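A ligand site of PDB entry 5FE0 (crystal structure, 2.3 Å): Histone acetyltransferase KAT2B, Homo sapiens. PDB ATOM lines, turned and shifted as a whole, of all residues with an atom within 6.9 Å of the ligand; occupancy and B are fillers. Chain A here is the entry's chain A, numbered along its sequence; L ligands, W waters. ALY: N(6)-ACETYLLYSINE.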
ATOM      1  N   PRO A  35      24.322  11.236 -27.094  1.00  0.00           N
ATOM      2  CA  PRO A  35      24.096   9.854 -26.588  1.00  0.00           C
ATOM      3  C   PRO A  35      23.019   9.692 -25.554  1.00  0.00           C
ATOM      4  O   PRO A  35      22.587   8.561 -25.335  1.00  0.00           O
ATOM      5  CB  PRO A  35      25.426   9.521 -25.886  1.00  0.00           C
ATOM      6  CG  PRO A  35      26.406  10.448 -26.504  1.00  0.00           C
ATOM      7  CD  PRO A  35      25.654  11.721 -26.705  1.00  0.00           C
ATOM      8  N   PHE A  36      22.595  10.784 -24.906  1.00  0.00           N
ATOM      9  CA  PHE A  36      21.756  10.733 -23.736  1.00  0.00           C
ATOM     10  C   PHE A  36      20.363  11.291 -23.962  1.00  0.00           C
ATOM     11  O   PHE A  36      19.617  11.476 -22.997  1.00  0.00           O
ATOM     12  CB  PHE A  36      22.408  11.557 -22.617  1.00  0.00           C
ATOM     13  CG  PHE A  36      23.879  11.304 -22.484  1.00  0.00           C
ATOM     14  CD1 PHE A  36      24.350  10.056 -22.063  1.00  0.00           C
ATOM     15  CD2 PHE A  36      24.816  12.276 -22.853  1.00  0.00           C
ATOM     16  CE1 PHE A  36      25.691   9.808 -21.961  1.00  0.00           C
ATOM     17  CE2 PHE A  36      26.171  12.026 -22.719  1.00  0.00           C
ATOM     18  CZ  PHE A  36      26.611  10.808 -22.251  1.00  0.00           C
ATOM     19  N   GLU A  38      17.574  10.120 -25.518  1.00  0.00           N
ATOM     20  CA  GLU A  38      16.458   9.230 -25.318  1.00  0.00           C
ATOM     21  C   GLU A  38      16.925   8.002 -24.578  1.00  0.00           C
ATOM     22  O   GLU A  38      18.120   7.753 -24.506  1.00  0.00           O
ATOM     23  CB  GLU A  38      15.868   8.862 -26.684  1.00  0.00           C
ATOM     24  CG  GLU A  38      15.154  10.039 -27.312  1.00  0.00           C
ATOM     25  CD  GLU A  38      14.456   9.718 -28.615  1.00  0.00           C
ATOM     26  OE1 GLU A  38      14.747   8.667 -29.253  1.00  0.00           O
ATOM     27  OE2 GLU A  38      13.572  10.547 -28.986  1.00  0.00           O
ATOM     28  N   VAL A  40      18.302   4.522 -23.764  1.00  0.00           N
ATOM     29  CA  VAL A  40      19.174   3.627 -24.529  1.00  0.00           C
ATOM     30  C   VAL A  40      18.328   2.556 -25.267  1.00  0.00           C
ATOM     31  O   VAL A  40      17.454   1.941 -24.659  1.00  0.00           O
ATOM     32  CB  VAL A  40      20.231   2.996 -23.603  1.00  0.00           C
ATOM     33  CG1 VAL A  40      20.972   1.886 -24.285  1.00  0.00           C
ATOM     34  CG2 VAL A  40      21.203   4.074 -23.141  1.00  0.00           C
ATOM     35  N   LYS A  41      18.556   2.400 -26.564  1.00  0.00           N
ATOM     36  CA  LYS A  41      17.827   1.388 -27.395  1.00  0.00           C
ATOM     37  C   LYS A  41      18.506   0.020 -27.294  1.00  0.00           C
ATOM     38  O   LYS A  41      19.717  -0.089 -27.430  1.00  0.00           O
ATOM     39  CB  LYS A  41      17.739   1.860 -28.839  1.00  0.00           C
ATOM     40  CG  LYS A  41      17.087   3.224 -29.003  1.00  0.00           C
ATOM     41  CD  LYS A  41      16.888   3.605 -30.441  1.00  0.00           C
ATOM     42  CE  LYS A  41      16.083   4.870 -30.638  1.00  0.00           C
ATOM     43  NZ  LYS A  41      16.380   6.003 -29.698  1.00  0.00           N
ATOM     44  N   ARG A  42      17.718  -1.024 -27.064  1.00  0.00           N
ATOM     45  CA  ARG A  42      18.235  -2.444 -27.078  1.00  0.00           C
ATOM     46  C   ARG A  42      18.974  -2.792 -28.352  1.00  0.00           C
ATOM     47  O   ARG A  42      19.941  -3.536 -28.329  1.00  0.00           O
ATOM     48  CB  ARG A  42      17.132  -3.436 -26.921  1.00  0.00           C
ATOM     49  CG  ARG A  42      16.609  -3.565 -25.517  1.00  0.00           C
ATOM     50  CD  ARG A  42      15.270  -4.246 -25.497  1.00  0.00           C
ATOM     51  NE  ARG A  42      14.580  -4.007 -24.237  1.00  0.00           N
ATOM     52  CZ  ARG A  42      14.906  -4.554 -23.048  1.00  0.00           C
ATOM     53  NH1 ARG A  42      14.205  -4.211 -21.967  1.00  0.00           N
ATOM     54  NH2 ARG A  42      15.912  -5.437 -22.936  1.00  0.00           N
ATOM     55  N   THR A  43      18.497  -2.273 -29.477  1.00  0.00           N
ATOM     56  CA  THR A  43      19.112  -2.572 -30.757  1.00  0.00           C
ATOM     57  C   THR A  43      20.515  -1.979 -30.848  1.00  0.00           C
ATOM     58  O   THR A  43      21.369  -2.507 -31.527  1.00  0.00           O
ATOM     59  CB  THR A  43      18.275  -2.015 -31.910  1.00  0.00           C
ATOM     60  OG1 THR A  43      18.135  -0.597 -31.766  1.00  0.00           O
ATOM     61  CG2 THR A  43      16.915  -2.665 -31.924  1.00  0.00           C
ATOM     62  N   GLU A  44      20.744  -0.872 -30.145  1.00  0.00           N
ATOM     63  CA  GLU A  44      22.093  -0.309 -30.094  1.00  0.00           C
ATOM     64  C   GLU A  44      22.962  -0.984 -29.044  1.00  0.00           C
ATOM     65  O   GLU A  44      24.150  -1.098 -29.233  1.00  0.00           O
ATOM     66  CB  GLU A  44      22.032   1.203 -29.834  1.00  0.00           C
ATOM     67  CG  GLU A  44      21.389   2.036 -30.955  1.00  0.00           C
ATOM     68  CD  GLU A  44      21.230   3.544 -30.601  1.00  0.00           C
ATOM     69  OE1 GLU A  44      21.752   3.953 -29.513  1.00  0.00           O
ATOM     70  OE2 GLU A  44      20.617   4.305 -31.418  1.00  0.00           O
ATOM     71  N   ALA A  45      22.372  -1.423 -27.944  1.00  0.00           N
ATOM     72  CA  ALA A  45      23.089  -1.926 -26.805  1.00  0.00           C
ATOM     73  C   ALA A  45      22.307  -3.184 -26.255  1.00  0.00           C
ATOM     74  O   ALA A  45      21.566  -3.094 -25.285  1.00  0.00           O
ATOM     75  CB  ALA A  45      23.149  -0.842 -25.745  1.00  0.00           C
ATOM     76  N   PRO A  46      22.432  -4.330 -26.908  1.00  0.00           N
ATOM     77  CA  PRO A  46      21.528  -5.479 -26.595  1.00  0.00           C
ATOM     78  C   PRO A  46      21.363  -5.922 -25.114  1.00  0.00           C
ATOM     79  O   PRO A  46      20.226  -6.238 -24.701  1.00  0.00           O
ATOM     80  CB  PRO A  46      22.085  -6.620 -27.444  1.00  0.00           C
ATOM     81  CG  PRO A  46      22.877  -5.966 -28.538  1.00  0.00           C
ATOM     82  CD  PRO A  46      23.184  -4.536 -28.155  1.00  0.00           C
ATOM     83  N   GLY A  47      22.443  -5.949 -24.334  1.00  0.00           N
ATOM     84  CA  GLY A  47      22.363  -6.371 -22.908  1.00  0.00           C
ATOM     85  C   GLY A  47      22.441  -5.271 -21.880  1.00  0.00           C
ATOM     86  O   GLY A  47      22.912  -5.494 -20.774  1.00  0.00           O
ATOM     87  N   TYR A  48      22.039  -4.077 -22.278  1.00  0.00           N
ATOM     88  CA  TYR A  48      22.180  -2.857 -21.454  1.00  0.00           C
ATOM     89  C   TYR A  48      21.306  -2.900 -20.225  1.00  0.00           C
ATOM     90  O   TYR A  48      21.765  -2.603 -19.090  1.00  0.00           O
ATOM     91  CB  TYR A  48      21.806  -1.613 -22.285  1.00  0.00           C
ATOM     92  CG  TYR A  48      21.975  -0.289 -21.568  1.00  0.00           C
ATOM     93  CD1 TYR A  48      20.933   0.267 -20.830  1.00  0.00           C
ATOM     94  CD2 TYR A  48      23.187   0.381 -21.615  1.00  0.00           C
ATOM     95  CE1 TYR A  48      21.105   1.485 -20.165  1.00  0.00           C
ATOM     96  CE2 TYR A  48      23.358   1.599 -20.950  1.00  0.00           C
ATOM     97  CZ  TYR A  48      22.321   2.143 -20.215  1.00  0.00           C
ATOM     98  OH  TYR A  48      22.508   3.369 -19.587  1.00  0.00           O
ATOM     99  N   MET A  56      18.525   6.305 -17.073  1.00  0.00           N
ATOM    100  CA  MET A  56      18.056   7.672 -17.084  1.00  0.00           C
ATOM    101  C   MET A  56      18.534   8.329 -18.362  1.00  0.00           C
ATOM    102  O   MET A  56      19.562   7.965 -18.912  1.00  0.00           O
ATOM    103  CB  MET A  56      18.550   8.447 -15.829  1.00  0.00           C
ATOM    104  CG  MET A  56      17.948   9.837 -15.603  1.00  0.00           C
ATOM    105  SD  MET A  56      16.163   9.941 -15.884  1.00  0.00           S
ATOM    106  CE  MET A  56      15.598   8.743 -14.662  1.00  0.00           C
ATOM    107  N   VAL A  83      22.618   9.692 -15.325  1.00  0.00           N
ATOM    108  CA  VAL A  83      22.912   9.641 -16.734  1.00  0.00           C
ATOM    109  C   VAL A  83      24.405   9.395 -16.932  1.00  0.00           C
ATOM    110  O   VAL A  83      24.798   8.563 -17.754  1.00  0.00           O
ATOM    111  CB  VAL A  83      22.454  10.918 -17.494  1.00  0.00           C
ATOM    112  CG1 VAL A  83      22.865  10.856 -18.968  1.00  0.00           C
ATOM    113  CG2 VAL A  83      20.951  11.082 -17.428  1.00  0.00           C
ATOM    114  N   ASN A  86      25.785   5.870 -15.218  1.00  0.00           N
ATOM    115  CA  ASN A  86      25.376   4.735 -16.096  1.00  0.00           C
ATOM    116  C   ASN A  86      26.302   4.609 -17.257  1.00  0.00           C
ATOM    117  O   ASN A  86      26.821   3.515 -17.518  1.00  0.00           O
ATOM    118  CB  ASN A  86      23.976   4.917 -16.638  1.00  0.00           C
ATOM    119  CG  ASN A  86      22.914   4.725 -15.587  1.00  0.00           C
ATOM    120  OD1 ASN A  86      23.201   4.220 -14.473  1.00  0.00           O
ATOM    121  ND2 ASN A  86      21.691   5.126 -15.896  1.00  0.00           N
ATOM    122  N   CYS A  87      26.548   5.732 -17.932  1.00  0.00           N
ATOM    123  CA  CYS A  87      27.366   5.760 -19.112  1.00  0.00           C
ATOM    124  C   CYS A  87      28.791   5.358 -18.816  1.00  0.00           C
ATOM    125  O   CYS A  87      29.390   4.617 -19.603  1.00  0.00           O
ATOM    126  CB  CYS A  87      27.304   7.146 -19.762  1.00  0.00           C
ATOM    127  SG  CYS A  87      28.418   7.368 -21.156  1.00  0.00           S
ATOM    128  N   LYS A  88      29.330   5.772 -17.690  1.00  0.00           N
ATOM    129  CA  LYS A  88      30.699   5.414 -17.354  1.00  0.00           C
ATOM    130  C   LYS A  88      30.867   3.999 -16.809  1.00  0.00           C
ATOM    131  O   LYS A  88      31.920   3.395 -16.992  1.00  0.00           O
ATOM    132  CB  LYS A  88      31.243   6.418 -16.379  1.00  0.00           C
ATOM    133  CG  LYS A  88      31.388   7.796 -16.982  1.00  0.00           C
ATOM    134  CD  LYS A  88      31.691   8.683 -15.787  1.00  0.00           C
ATOM    135  CE  LYS A  88      31.824  10.109 -16.161  1.00  0.00           C
ATOM    136  NZ  LYS A  88      31.897  10.918 -14.933  1.00  0.00           N
ATOM    137  N   TYR A  90      28.897   1.481 -18.040  1.00  0.00           N
ATOM    138  CA  TYR A  90      28.647   0.605 -19.187  1.00  0.00           C
ATOM    139  C   TYR A  90      29.740   0.660 -20.240  1.00  0.00           C
ATOM    140  O   TYR A  90      30.104  -0.353 -20.807  1.00  0.00           O
ATOM    141  CB  TYR A  90      27.296   0.929 -19.830  1.00  0.00           C
ATOM    142  CG  TYR A  90      26.880  -0.094 -20.843  1.00  0.00           C
ATOM    143  CD1 TYR A  90      26.454  -1.361 -20.452  1.00  0.00           C
ATOM    144  CD2 TYR A  90      26.922   0.202 -22.216  1.00  0.00           C
ATOM    145  CE1 TYR A  90      26.097  -2.317 -21.411  1.00  0.00           C
ATOM    146  CE2 TYR A  90      26.582  -0.763 -23.171  1.00  0.00           C
ATOM    147  CZ  TYR A  90      26.161  -2.010 -22.755  1.00  0.00           C
ATOM    148  OH  TYR A  90      25.792  -2.954 -23.690  1.00  0.00           O
ATOM    149  N   ASN A  91      30.261   1.859 -20.514  1.00  0.00           N
ATOM    150  CA  ASN A  91      31.111   2.098 -21.683  1.00  0.00           C
ATOM    151  C   ASN A  91      32.608   2.156 -21.354  1.00  0.00           C
ATOM    152  O   ASN A  91      33.046   2.653 -20.293  1.00  0.00           O
ATOM    153  CB  ASN A  91      30.675   3.384 -22.377  1.00  0.00           C
ATOM    154  CG  ASN A  91      29.264   3.309 -22.928  1.00  0.00           C
ATOM    155  OD1 ASN A  91      29.061   2.767 -23.995  1.00  0.00           O
ATOM    156  ND2 ASN A  91      28.295   3.869 -22.235  1.00  0.00           N
ATOM    157  N   PRO A  92      33.441   1.653 -22.294  1.00  0.00           N
ATOM    158  CA  PRO A  92      34.900   1.751 -22.091  1.00  0.00           C
ATOM    159  C   PRO A  92      35.373   3.198 -21.893  1.00  0.00           C
ATOM    160  O   PRO A  92      34.793   4.119 -22.500  1.00  0.00           O
ATOM    161  CB  PRO A  92      35.484   1.139 -23.382  1.00  0.00           C
ATOM    162  CG  PRO A  92      34.358   0.426 -24.046  1.00  0.00           C
ATOM    163  CD  PRO A  92      33.096   1.108 -23.627  1.00  0.00           C
ATOM    164  N   TYR A  97      31.321   7.679 -25.981  1.00  0.00           N
ATOM    165  CA  TYR A  97      30.217   7.858 -25.055  1.00  0.00           C
ATOM    166  C   TYR A  97      30.738   8.362 -23.719  1.00  0.00           C
ATOM    167  O   TYR A  97      30.149   9.255 -23.137  1.00  0.00           O
ATOM    168  CB  TYR A  97      29.412   6.556 -24.814  1.00  0.00           C
ATOM    169  CG  TYR A  97      28.719   6.028 -26.043  1.00  0.00           C
ATOM    170  CD1 TYR A  97      27.646   6.696 -26.611  1.00  0.00           C
ATOM    171  CD2 TYR A  97      29.209   4.903 -26.697  1.00  0.00           C
ATOM    172  CE1 TYR A  97      27.055   6.225 -27.793  1.00  0.00           C
ATOM    173  CE2 TYR A  97      28.607   4.415 -27.831  1.00  0.00           C
ATOM    174  CZ  TYR A  97      27.543   5.048 -28.374  1.00  0.00           C
ATOM    175  OH  TYR A  97      26.974   4.530 -29.518  1.00  0.00           O
HETATM  176  OH  ALY L   1      25.617   4.591 -22.636  1.00  0.00           O
HETATM  177  CH  ALY L   1      24.973   5.094 -23.524  1.00  0.00           C
HETATM  178  CH3 ALY L   1      24.456   6.477 -23.367  1.00  0.00           C
HETATM  179  NZ  ALY L   1      24.703   4.474 -24.679  1.00  0.00           N
HETATM  180  CE  ALY L   1      25.094   3.099 -24.963  1.00  0.00           C
HETATM  181  CD  ALY L   1      25.937   2.944 -26.222  1.00  0.00           C
HETATM  182  CG  ALY L   1      26.039   1.488 -26.693  1.00  0.00           C
HETATM  183  CB  ALY L   1      27.393   1.269 -27.366  1.00  0.00           C
HETATM  184  CA  ALY L   1      27.605  -0.099 -28.019  1.00  0.00           C
HETATM  185  N   ALY L   1      26.678  -0.257 -29.180  1.00  0.00           N
HETATM  186  C   ALY L   1      27.411  -1.214 -27.038  1.00  0.00           C
HETATM  187  O   ALY L   1      28.153  -1.354 -26.065  1.00  0.00           O
HETATM  188  OXT ALY L   1      26.507  -2.039 -27.187  1.00  0.00           O
HETATM  189  O   HOH W   1      30.386  -1.756 -23.793  1.00  0.00           O
HETATM  190  O   HOH W   2      28.287   2.003 -30.718  1.00  0.00           O
HETATM  191  O   HOH W   3      30.436   0.418 -25.881  1.00  0.00           O
HETATM  192  O   HOH W   4      23.046   6.133 -26.481  1.00  0.00           O
HETATM  193  O   HOH W   5      24.413   4.747 -20.170  1.00  0.00           O
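O of Glu 44 sits at hydrogen-bond distance from N of the ligand, 2.7 Å away. An oxygen (OH) of the ligand is in hydrogen-bond range of the side-chain amide nitrogen of Asn 91 (2.8 Å).
ND2 of Asn 91 sits at hydrogen-bond distance from O of Cys 87 (2.9 Å). The side-chain sulfur (SG) of Cys 87 is in hydrogen-bond range of the backbone carbonyl oxygen (O) of Tyr 97.
Residues that only touch the ligand: Pro 35, Phe 36, Val 40, Ala 45, Tyr 90 and Tyr 97. Hydrophobic or aromatic side chains that line the ligand: Phe 36, Val 40, Ala 45, Tyr 90 and Tyr 97. Of the 21 residues printed, 8 come within 4 Å of the ligand.
Water W5 lies within hydrogen-bond range of OH of Tyr 48 (2.4 Å), OH of the ligand (2.7 Å) and N of Cys 87 (3.2 Å). Water W3 lies within hydrogen-bond range of O of the ligand (2.9 Å) and OD1 of Asn 91 (3.3 Å). Water W4 lies within hydrogen-bond range of O of Pro 35 and NZ of the ligand. Water W2 bridges the side-chain hydroxyl (OH) of Tyr 97 and a nitrogen (N) of the ligand. Water W1 bridges O of the ligand and O of Tyr 90.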
